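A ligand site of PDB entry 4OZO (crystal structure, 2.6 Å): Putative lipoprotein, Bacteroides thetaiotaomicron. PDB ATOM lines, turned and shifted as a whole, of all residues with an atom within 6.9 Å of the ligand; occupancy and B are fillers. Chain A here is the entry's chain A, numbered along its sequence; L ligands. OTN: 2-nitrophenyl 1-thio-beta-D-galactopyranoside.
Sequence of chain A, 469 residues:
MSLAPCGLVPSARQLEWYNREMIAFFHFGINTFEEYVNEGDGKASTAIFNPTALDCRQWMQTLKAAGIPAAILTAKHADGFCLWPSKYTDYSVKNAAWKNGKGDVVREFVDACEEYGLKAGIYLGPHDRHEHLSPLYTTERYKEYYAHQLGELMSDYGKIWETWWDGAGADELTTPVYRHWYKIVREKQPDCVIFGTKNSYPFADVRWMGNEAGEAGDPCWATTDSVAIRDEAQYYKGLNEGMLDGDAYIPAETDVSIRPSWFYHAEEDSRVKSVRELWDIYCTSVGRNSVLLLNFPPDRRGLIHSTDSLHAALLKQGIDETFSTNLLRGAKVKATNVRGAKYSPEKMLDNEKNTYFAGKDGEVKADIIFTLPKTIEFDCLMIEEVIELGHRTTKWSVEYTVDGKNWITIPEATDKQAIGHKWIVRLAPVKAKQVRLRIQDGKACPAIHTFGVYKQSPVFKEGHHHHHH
Merely in contact with the ligand: Thr 197, Trp 208, Ala 168, Trp 164 and Lys 198.
Ten residues have an atom within 4 Å of the ligand: Trp 164, Asp 166, Gly 167, Ala 168, Thr 197, Lys 198, Trp 208, Glu 212, Glu 232 and Asp 255.
The side-chain carboxylate (OD1) of Asp 166 is in hydrogen-bond range of the backbone NH (N) of Ala 168 (3.0 Å).
The side-chain carboxylate (OD2) of Asp 166 sits at hydrogen-bond distance from the side-chain hydroxyl (OH) of Tyr 123, at 2.6 Å.
The indole nitrogen (NE1) of Trp 262 lies within hydrogen-bond range of the side-chain carboxylate (OE1) of Glu 212 (3.1 Å).
The side-chain carboxylate of Asp 255 lies within hydrogen-bond range of the indole nitrogen of Trp 208 (2.9 Å).
The backbone carbonyl oxygen (O) of Gly 167 sits at hydrogen-bond distance from the side-chain amino group (NZ) of Lys 198.
The side-chain hydroxyl (OG1) of Thr 197 is in hydrogen-bond range of the backbone carbonyl oxygen (O) of Trp 165 (2.6 Å).
NE1 of Trp 208 is in hydrogen-bond range of O of Asn 211 (3.2 Å).
N of Lys 198 sits at hydrogen-bond distance from O of Ile 229.
An oxygen (O4) of the ligand is in hydrogen-bond range of the side-chain carboxylate (OD1) of Asp 166 (2.4 Å).
O6 of the ligand is in hydrogen-bond range of OE2 of Glu 212 (2.5 Å).
The side-chain carboxylate (OE1) of Glu 232 sits at hydrogen-bond distance from an oxygen (O2) of the ligand (2.5 Å).
An oxygen (O6) of the ligand sits at hydrogen-bond distance from the side-chain carboxylate (OD2) of Asp 255, at 2.6 Å.
The backbone NH of Gly 167 sits at hydrogen-bond distance from an oxygen (O4) of the ligand (3.0 Å).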
ATOM      1  N   PHE A  25      12.201 -20.497 -27.999  1.00  0.00           N
ATOM      2  CA  PHE A  25      11.606 -19.189 -28.152  1.00  0.00           C
ATOM      3  C   PHE A  25      11.912 -18.744 -29.580  1.00  0.00           C
ATOM      4  O   PHE A  25      12.987 -19.038 -30.110  1.00  0.00           O
ATOM      5  CB  PHE A  25      12.290 -18.209 -27.198  1.00  0.00           C
ATOM      6  CG  PHE A  25      11.344 -17.465 -26.289  1.00  0.00           C
ATOM      7  CD1 PHE A  25      10.021 -17.248 -26.641  1.00  0.00           C
ATOM      8  CD2 PHE A  25      11.803 -16.954 -25.074  1.00  0.00           C
ATOM      9  CE1 PHE A  25       9.161 -16.545 -25.791  1.00  0.00           C
ATOM     10  CE2 PHE A  25      10.957 -16.252 -24.220  1.00  0.00           C
ATOM     11  CZ  PHE A  25       9.628 -16.041 -24.577  1.00  0.00           C
ATOM     12  N   TYR A 123       3.462 -16.163 -27.050  1.00  0.00           N
ATOM     13  CA  TYR A 123       3.876 -15.030 -26.233  1.00  0.00           C
ATOM     14  C   TYR A 123       3.068 -13.829 -26.717  1.00  0.00           C
ATOM     15  O   TYR A 123       3.267 -13.365 -27.848  1.00  0.00           O
ATOM     16  CB  TYR A 123       5.367 -14.797 -26.398  1.00  0.00           C
ATOM     17  CG  TYR A 123       5.980 -13.532 -25.797  1.00  0.00           C
ATOM     18  CD1 TYR A 123       7.004 -13.619 -24.857  1.00  0.00           C
ATOM     19  CD2 TYR A 123       5.590 -12.265 -26.201  1.00  0.00           C
ATOM     20  CE1 TYR A 123       7.594 -12.490 -24.323  1.00  0.00           C
ATOM     21  CE2 TYR A 123       6.159 -11.130 -25.668  1.00  0.00           C
ATOM     22  CZ  TYR A 123       7.160 -11.244 -24.725  1.00  0.00           C
ATOM     23  OH  TYR A 123       7.745 -10.104 -24.198  1.00  0.00           O
ATOM     24  N   TRP A 164       2.632 -17.037 -22.554  1.00  0.00           N
ATOM     25  CA  TRP A 164       3.738 -16.386 -21.869  1.00  0.00           C
ATOM     26  C   TRP A 164       3.367 -14.939 -21.578  1.00  0.00           C
ATOM     27  O   TRP A 164       3.026 -14.177 -22.497  1.00  0.00           O
ATOM     28  CB  TRP A 164       4.989 -16.401 -22.752  1.00  0.00           C
ATOM     29  CG  TRP A 164       6.251 -16.818 -22.069  1.00  0.00           C
ATOM     30  CD1 TRP A 164       6.636 -18.098 -21.767  1.00  0.00           C
ATOM     31  CD2 TRP A 164       7.316 -15.968 -21.626  1.00  0.00           C
ATOM     32  NE1 TRP A 164       7.870 -18.091 -21.154  1.00  0.00           N
ATOM     33  CE2 TRP A 164       8.323 -16.796 -21.065  1.00  0.00           C
ATOM     34  CE3 TRP A 164       7.521 -14.577 -21.651  1.00  0.00           C
ATOM     35  CZ2 TRP A 164       9.507 -16.297 -20.536  1.00  0.00           C
ATOM     36  CZ3 TRP A 164       8.705 -14.077 -21.122  1.00  0.00           C
ATOM     37  CH2 TRP A 164       9.677 -14.945 -20.569  1.00  0.00           C
ATOM     38  N   TRP A 165       3.431 -14.581 -20.300  1.00  0.00           N
ATOM     39  CA  TRP A 165       3.148 -13.220 -19.869  1.00  0.00           C
ATOM     40  C   TRP A 165       4.412 -12.573 -19.300  1.00  0.00           C
ATOM     41  O   TRP A 165       4.700 -12.681 -18.111  1.00  0.00           O
ATOM     42  CB  TRP A 165       2.007 -13.220 -18.840  1.00  0.00           C
ATOM     43  CG  TRP A 165       0.679 -13.525 -19.451  1.00  0.00           C
ATOM     44  CD1 TRP A 165       0.350 -13.433 -20.774  1.00  0.00           C
ATOM     45  CD2 TRP A 165      -0.503 -13.976 -18.767  1.00  0.00           C
ATOM     46  NE1 TRP A 165      -0.964 -13.795 -20.959  1.00  0.00           N
ATOM     47  CE2 TRP A 165      -1.516 -14.133 -19.743  1.00  0.00           C
ATOM     48  CE3 TRP A 165      -0.805 -14.265 -17.440  1.00  0.00           C
ATOM     49  CZ2 TRP A 165      -2.807 -14.560 -19.423  1.00  0.00           C
ATOM     50  CZ3 TRP A 165      -2.096 -14.692 -17.119  1.00  0.00           C
ATOM     51  CH2 TRP A 165      -3.075 -14.835 -18.115  1.00  0.00           C
ATOM     52  N   ASP A 166       5.167 -11.935 -20.187  1.00  0.00           N
ATOM     53  CA  ASP A 166       6.300 -11.098 -19.814  1.00  0.00           C
ATOM     54  C   ASP A 166       5.835 -10.024 -18.828  1.00  0.00           C
ATOM     55  O   ASP A 166       4.747  -9.454 -18.979  1.00  0.00           O
ATOM     56  CB  ASP A 166       6.847 -10.440 -21.080  1.00  0.00           C
ATOM     57  CG  ASP A 166       8.252  -9.878 -20.892  1.00  0.00           C
ATOM     58  OD1 ASP A 166       8.635  -9.599 -19.739  1.00  0.00           O
ATOM     59  OD2 ASP A 166       8.957  -9.721 -21.911  1.00  0.00           O
ATOM     60  N   GLY A 167       6.680  -9.723 -17.840  1.00  0.00           N
ATOM     61  CA  GLY A 167       6.315  -8.761 -16.819  1.00  0.00           C
ATOM     62  C   GLY A 167       6.904  -7.375 -17.020  1.00  0.00           C
ATOM     63  O   GLY A 167       6.576  -6.456 -16.281  1.00  0.00           O
ATOM     64  N   ALA A 168       7.771  -7.235 -18.019  1.00  0.00           N
ATOM     65  CA  ALA A 168       8.347  -5.932 -18.325  1.00  0.00           C
ATOM     66  C   ALA A 168       7.246  -4.887 -18.629  1.00  0.00           C
ATOM     67  O   ALA A 168       6.346  -5.122 -19.445  1.00  0.00           O
ATOM     68  CB  ALA A 168       9.343  -6.040 -19.484  1.00  0.00           C
ATOM     69  N   GLY A 169       7.319  -3.748 -17.940  1.00  0.00           N
ATOM     70  CA  GLY A 169       6.378  -2.663 -18.148  1.00  0.00           C
ATOM     71  C   GLY A 169       4.931  -3.020 -17.840  1.00  0.00           C
ATOM     72  O   GLY A 169       4.037  -2.252 -18.184  1.00  0.00           O
ATOM     73  N   PHE A 195       3.043 -19.092 -18.256  1.00  0.00           N
ATOM     74  CA  PHE A 195       4.182 -18.429 -17.650  1.00  0.00           C
ATOM     75  C   PHE A 195       3.705 -17.098 -17.075  1.00  0.00           C
ATOM     76  O   PHE A 195       3.360 -16.189 -17.846  1.00  0.00           O
ATOM     77  CB  PHE A 195       5.262 -18.187 -18.681  1.00  0.00           C
ATOM     78  CG  PHE A 195       6.477 -17.466 -18.141  1.00  0.00           C
ATOM     79  CD1 PHE A 195       7.526 -18.172 -17.563  1.00  0.00           C
ATOM     80  CD2 PHE A 195       6.585 -16.092 -18.247  1.00  0.00           C
ATOM     81  CE1 PHE A 195       8.646 -17.513 -17.092  1.00  0.00           C
ATOM     82  CE2 PHE A 195       7.700 -15.423 -17.783  1.00  0.00           C
ATOM     83  CZ  PHE A 195       8.733 -16.133 -17.199  1.00  0.00           C
ATOM     84  N   GLY A 196       3.667 -16.981 -15.754  1.00  0.00           N
ATOM     85  CA  GLY A 196       3.136 -15.791 -15.118  1.00  0.00           C
ATOM     86  C   GLY A 196       4.154 -14.963 -14.360  1.00  0.00           C
ATOM     87  O   GLY A 196       4.976 -15.478 -13.608  1.00  0.00           O
ATOM     88  N   THR A 197       4.078 -13.644 -14.553  1.00  0.00           N
ATOM     89  CA  THR A 197       4.894 -12.712 -13.790  1.00  0.00           C
ATOM     90  C   THR A 197       4.038 -11.663 -13.054  1.00  0.00           C
ATOM     91  O   THR A 197       2.928 -11.323 -13.462  1.00  0.00           O
ATOM     92  CB  THR A 197       5.911 -12.009 -14.704  1.00  0.00           C
ATOM     93  OG1 THR A 197       5.225 -11.444 -15.838  1.00  0.00           O
ATOM     94  CG2 THR A 197       6.944 -12.985 -15.205  1.00  0.00           C
ATOM     95  N   LYS A 198       4.592 -11.154 -11.956  1.00  0.00           N
ATOM     96  CA  LYS A 198       3.985 -10.067 -11.196  1.00  0.00           C
ATOM     97  C   LYS A 198       2.517 -10.300 -10.792  1.00  0.00           C
ATOM     98  O   LYS A 198       2.196 -11.318 -10.164  1.00  0.00           O
ATOM     99  CB  LYS A 198       4.190  -8.763 -11.955  1.00  0.00           C
ATOM    100  CG  LYS A 198       5.654  -8.554 -12.280  1.00  0.00           C
ATOM    101  CD  LYS A 198       5.944  -7.228 -12.971  1.00  0.00           C
ATOM    102  CE  LYS A 198       7.430  -6.926 -12.868  1.00  0.00           C
ATOM    103  NZ  LYS A 198       7.874  -5.793 -13.694  1.00  0.00           N
ATOM    104  N   TRP A 208       9.069 -17.146 -13.486  1.00  0.00           N
ATOM    105  CA  TRP A 208      10.395 -16.736 -13.889  1.00  0.00           C
ATOM    106  C   TRP A 208      11.380 -17.085 -12.774  1.00  0.00           C
ATOM    107  O   TRP A 208      10.958 -17.375 -11.640  1.00  0.00           O
ATOM    108  CB  TRP A 208      10.425 -15.214 -14.144  1.00  0.00           C
ATOM    109  CG  TRP A 208      11.708 -14.755 -14.763  1.00  0.00           C
ATOM    110  CD1 TRP A 208      12.492 -15.442 -15.659  1.00  0.00           C
ATOM    111  CD2 TRP A 208      12.376 -13.526 -14.516  1.00  0.00           C
ATOM    112  NE1 TRP A 208      13.581 -14.703 -15.990  1.00  0.00           N
ATOM    113  CE2 TRP A 208      13.546 -13.519 -15.302  1.00  0.00           C
ATOM    114  CE3 TRP A 208      12.089 -12.415 -13.722  1.00  0.00           C
ATOM    115  CZ2 TRP A 208      14.427 -12.445 -15.318  1.00  0.00           C
ATOM    116  CZ3 TRP A 208      12.975 -11.339 -13.724  1.00  0.00           C
ATOM    117  CH2 TRP A 208      14.129 -11.366 -14.510  1.00  0.00           C
ATOM    118  N   GLY A 210      14.426 -15.029 -12.315  1.00  0.00           N
ATOM    119  CA  GLY A 210      15.195 -13.882 -11.890  1.00  0.00           C
ATOM    120  C   GLY A 210      16.332 -13.351 -12.739  1.00  0.00           C
ATOM    121  O   GLY A 210      16.842 -12.265 -12.481  1.00  0.00           O
ATOM    122  N   ASN A 211      16.748 -14.117 -13.746  1.00  0.00           N
ATOM    123  CA  ASN A 211      17.748 -13.605 -14.663  1.00  0.00           C
ATOM    124  C   ASN A 211      17.558 -14.159 -16.067  1.00  0.00           C
ATOM    125  O   ASN A 211      16.709 -15.026 -16.292  1.00  0.00           O
ATOM    126  CB  ASN A 211      19.173 -13.879 -14.165  1.00  0.00           C
ATOM    127  CG  ASN A 211      19.493 -15.365 -14.095  1.00  0.00           C
ATOM    128  OD1 ASN A 211      19.833 -16.000 -15.108  1.00  0.00           O
ATOM    129  ND2 ASN A 211      19.399 -15.942 -12.894  1.00  0.00           N
ATOM    130  N   GLU A 212      18.356 -13.663 -16.996  1.00  0.00           N
ATOM    131  CA  GLU A 212      18.249 -14.095 -18.372  1.00  0.00           C
ATOM    132  C   GLU A 212      19.608 -14.603 -18.830  1.00  0.00           C
ATOM    133  O   GLU A 212      19.994 -14.400 -19.973  1.00  0.00           O
ATOM    134  CB  GLU A 212      17.764 -12.944 -19.268  1.00  0.00           C
ATOM    135  CG  GLU A 212      16.330 -12.543 -18.990  1.00  0.00           C
ATOM    136  CD  GLU A 212      15.863 -11.391 -19.870  1.00  0.00           C
ATOM    137  OE1 GLU A 212      16.706 -10.778 -20.551  1.00  0.00           O
ATOM    138  OE2 GLU A 212      14.636 -11.112 -19.886  1.00  0.00           O
ATOM    139  N   ILE A 229       6.651 -13.957  -6.825  1.00  0.00           N
ATOM    140  CA  ILE A 229       6.311 -13.662  -8.204  1.00  0.00           C
ATOM    141  C   ILE A 229       5.788 -12.231  -8.378  1.00  0.00           C
ATOM    142  O   ILE A 229       6.266 -11.476  -9.224  1.00  0.00           O
ATOM    143  CB  ILE A 229       5.274 -14.679  -8.720  1.00  0.00           C
ATOM    144  CG1 ILE A 229       5.873 -16.088  -8.713  1.00  0.00           C
ATOM    145  CG2 ILE A 229       4.729 -14.267 -10.087  1.00  0.00           C
ATOM    146  CD1 ILE A 229       4.855 -17.184  -8.824  1.00  0.00           C
ATOM    147  N   GLU A 232       8.442  -9.590  -7.539  1.00  0.00           N
ATOM    148  CA  GLU A 232       9.606  -9.942  -8.358  1.00  0.00           C
ATOM    149  C   GLU A 232      10.916  -9.204  -8.065  1.00  0.00           C
ATOM    150  O   GLU A 232      11.944  -9.821  -7.757  1.00  0.00           O
ATOM    151  CB  GLU A 232       9.212  -9.748  -9.828  1.00  0.00           C
ATOM    152  CG  GLU A 232      10.342  -9.788 -10.812  1.00  0.00           C
ATOM    153  CD  GLU A 232       9.862  -9.707 -12.237  1.00  0.00           C
ATOM    154  OE1 GLU A 232      10.467  -8.970 -13.038  1.00  0.00           O
ATOM    155  OE2 GLU A 232       8.859 -10.387 -12.562  1.00  0.00           O
ATOM    156  N   ASP A 255      14.886 -18.811 -19.074  1.00  0.00           N
ATOM    157  CA  ASP A 255      14.864 -18.271 -20.429  1.00  0.00           C
ATOM    158  C   ASP A 255      16.179 -17.601 -20.798  1.00  0.00           C
ATOM    159  O   ASP A 255      16.722 -16.819 -20.033  1.00  0.00           O
ATOM    160  CB  ASP A 255      13.686 -17.308 -20.633  1.00  0.00           C
ATOM    161  CG  ASP A 255      13.729 -16.095 -19.690  1.00  0.00           C
ATOM    162  OD1 ASP A 255      13.853 -16.283 -18.458  1.00  0.00           O
ATOM    163  OD2 ASP A 255      13.618 -14.943 -20.202  1.00  0.00           O
ATOM    164  N   TRP A 262      17.733 -10.649 -27.958  1.00  0.00           N
ATOM    165  CA  TRP A 262      16.577 -11.527 -28.149  1.00  0.00           C
ATOM    166  C   TRP A 262      16.120 -11.521 -29.608  1.00  0.00           C
ATOM    167  O   TRP A 262      15.682 -12.551 -30.133  1.00  0.00           O
ATOM    168  CB  TRP A 262      15.418 -11.132 -27.225  1.00  0.00           C
ATOM    169  CG  TRP A 262      15.625 -11.447 -25.773  1.00  0.00           C
ATOM    170  CD1 TRP A 262      15.955 -10.550 -24.778  1.00  0.00           C
ATOM    171  CD2 TRP A 262      15.499 -12.723 -25.131  1.00  0.00           C
ATOM    172  NE1 TRP A 262      16.040 -11.199 -23.571  1.00  0.00           N
ATOM    173  CE2 TRP A 262      15.769 -12.538 -23.755  1.00  0.00           C
ATOM    174  CE3 TRP A 262      15.192 -14.007 -25.585  1.00  0.00           C
ATOM    175  CZ2 TRP A 262      15.749 -13.586 -22.836  1.00  0.00           C
ATOM    176  CZ3 TRP A 262      15.164 -15.048 -24.664  1.00  0.00           C
ATOM    177  CH2 TRP A 262      15.442 -14.832 -23.316  1.00  0.00           C
HETATM  178  O2' OTN L   1      15.442  -4.398 -17.593  1.00  0.00           O
HETATM  179  N1' OTN L   1      14.454  -5.463 -17.494  1.00  0.00           N
HETATM  180  O3' OTN L   1      13.142  -5.140 -17.519  1.00  0.00           O
HETATM  181  C2' OTN L   1      14.910  -6.719 -17.394  1.00  0.00           C
HETATM  182  C3' OTN L   1      16.288  -6.923 -17.335  1.00  0.00           C
HETATM  183  C4' OTN L   1      16.826  -8.190 -17.244  1.00  0.00           C
HETATM  184  C5' OTN L   1      15.977  -9.284 -17.184  1.00  0.00           C
HETATM  185  C6' OTN L   1      14.606  -9.093 -17.213  1.00  0.00           C
HETATM  186  C1' OTN L   1      14.045  -7.824 -17.297  1.00  0.00           C
HETATM  187  S01 OTN L   1      12.306  -7.727 -17.376  1.00  0.00           S
HETATM  188  C1  OTN L   1      11.818  -9.368 -16.858  1.00  0.00           C
HETATM  189  O5  OTN L   1      11.948 -10.399 -17.904  1.00  0.00           O
HETATM  190  C5  OTN L   1      11.512 -11.665 -17.391  1.00  0.00           C
HETATM  191  C6  OTN L   1      11.687 -12.705 -18.501  1.00  0.00           C
HETATM  192  O6  OTN L   1      13.064 -12.773 -18.881  1.00  0.00           O
HETATM  193  C4  OTN L   1      10.043 -11.609 -16.960  1.00  0.00           C
HETATM  194  O4  OTN L   1       9.216 -11.249 -18.065  1.00  0.00           O
HETATM  195  C3  OTN L   1       9.938 -10.554 -15.895  1.00  0.00           C
HETATM  196  O3  OTN L   1       8.576 -10.419 -15.394  1.00  0.00           O
HETATM  197  C2  OTN L   1      10.383  -9.237 -16.505  1.00  0.00           C
HETATM  198  O2  OTN L   1      10.267  -8.283 -15.462  1.00  0.00           O
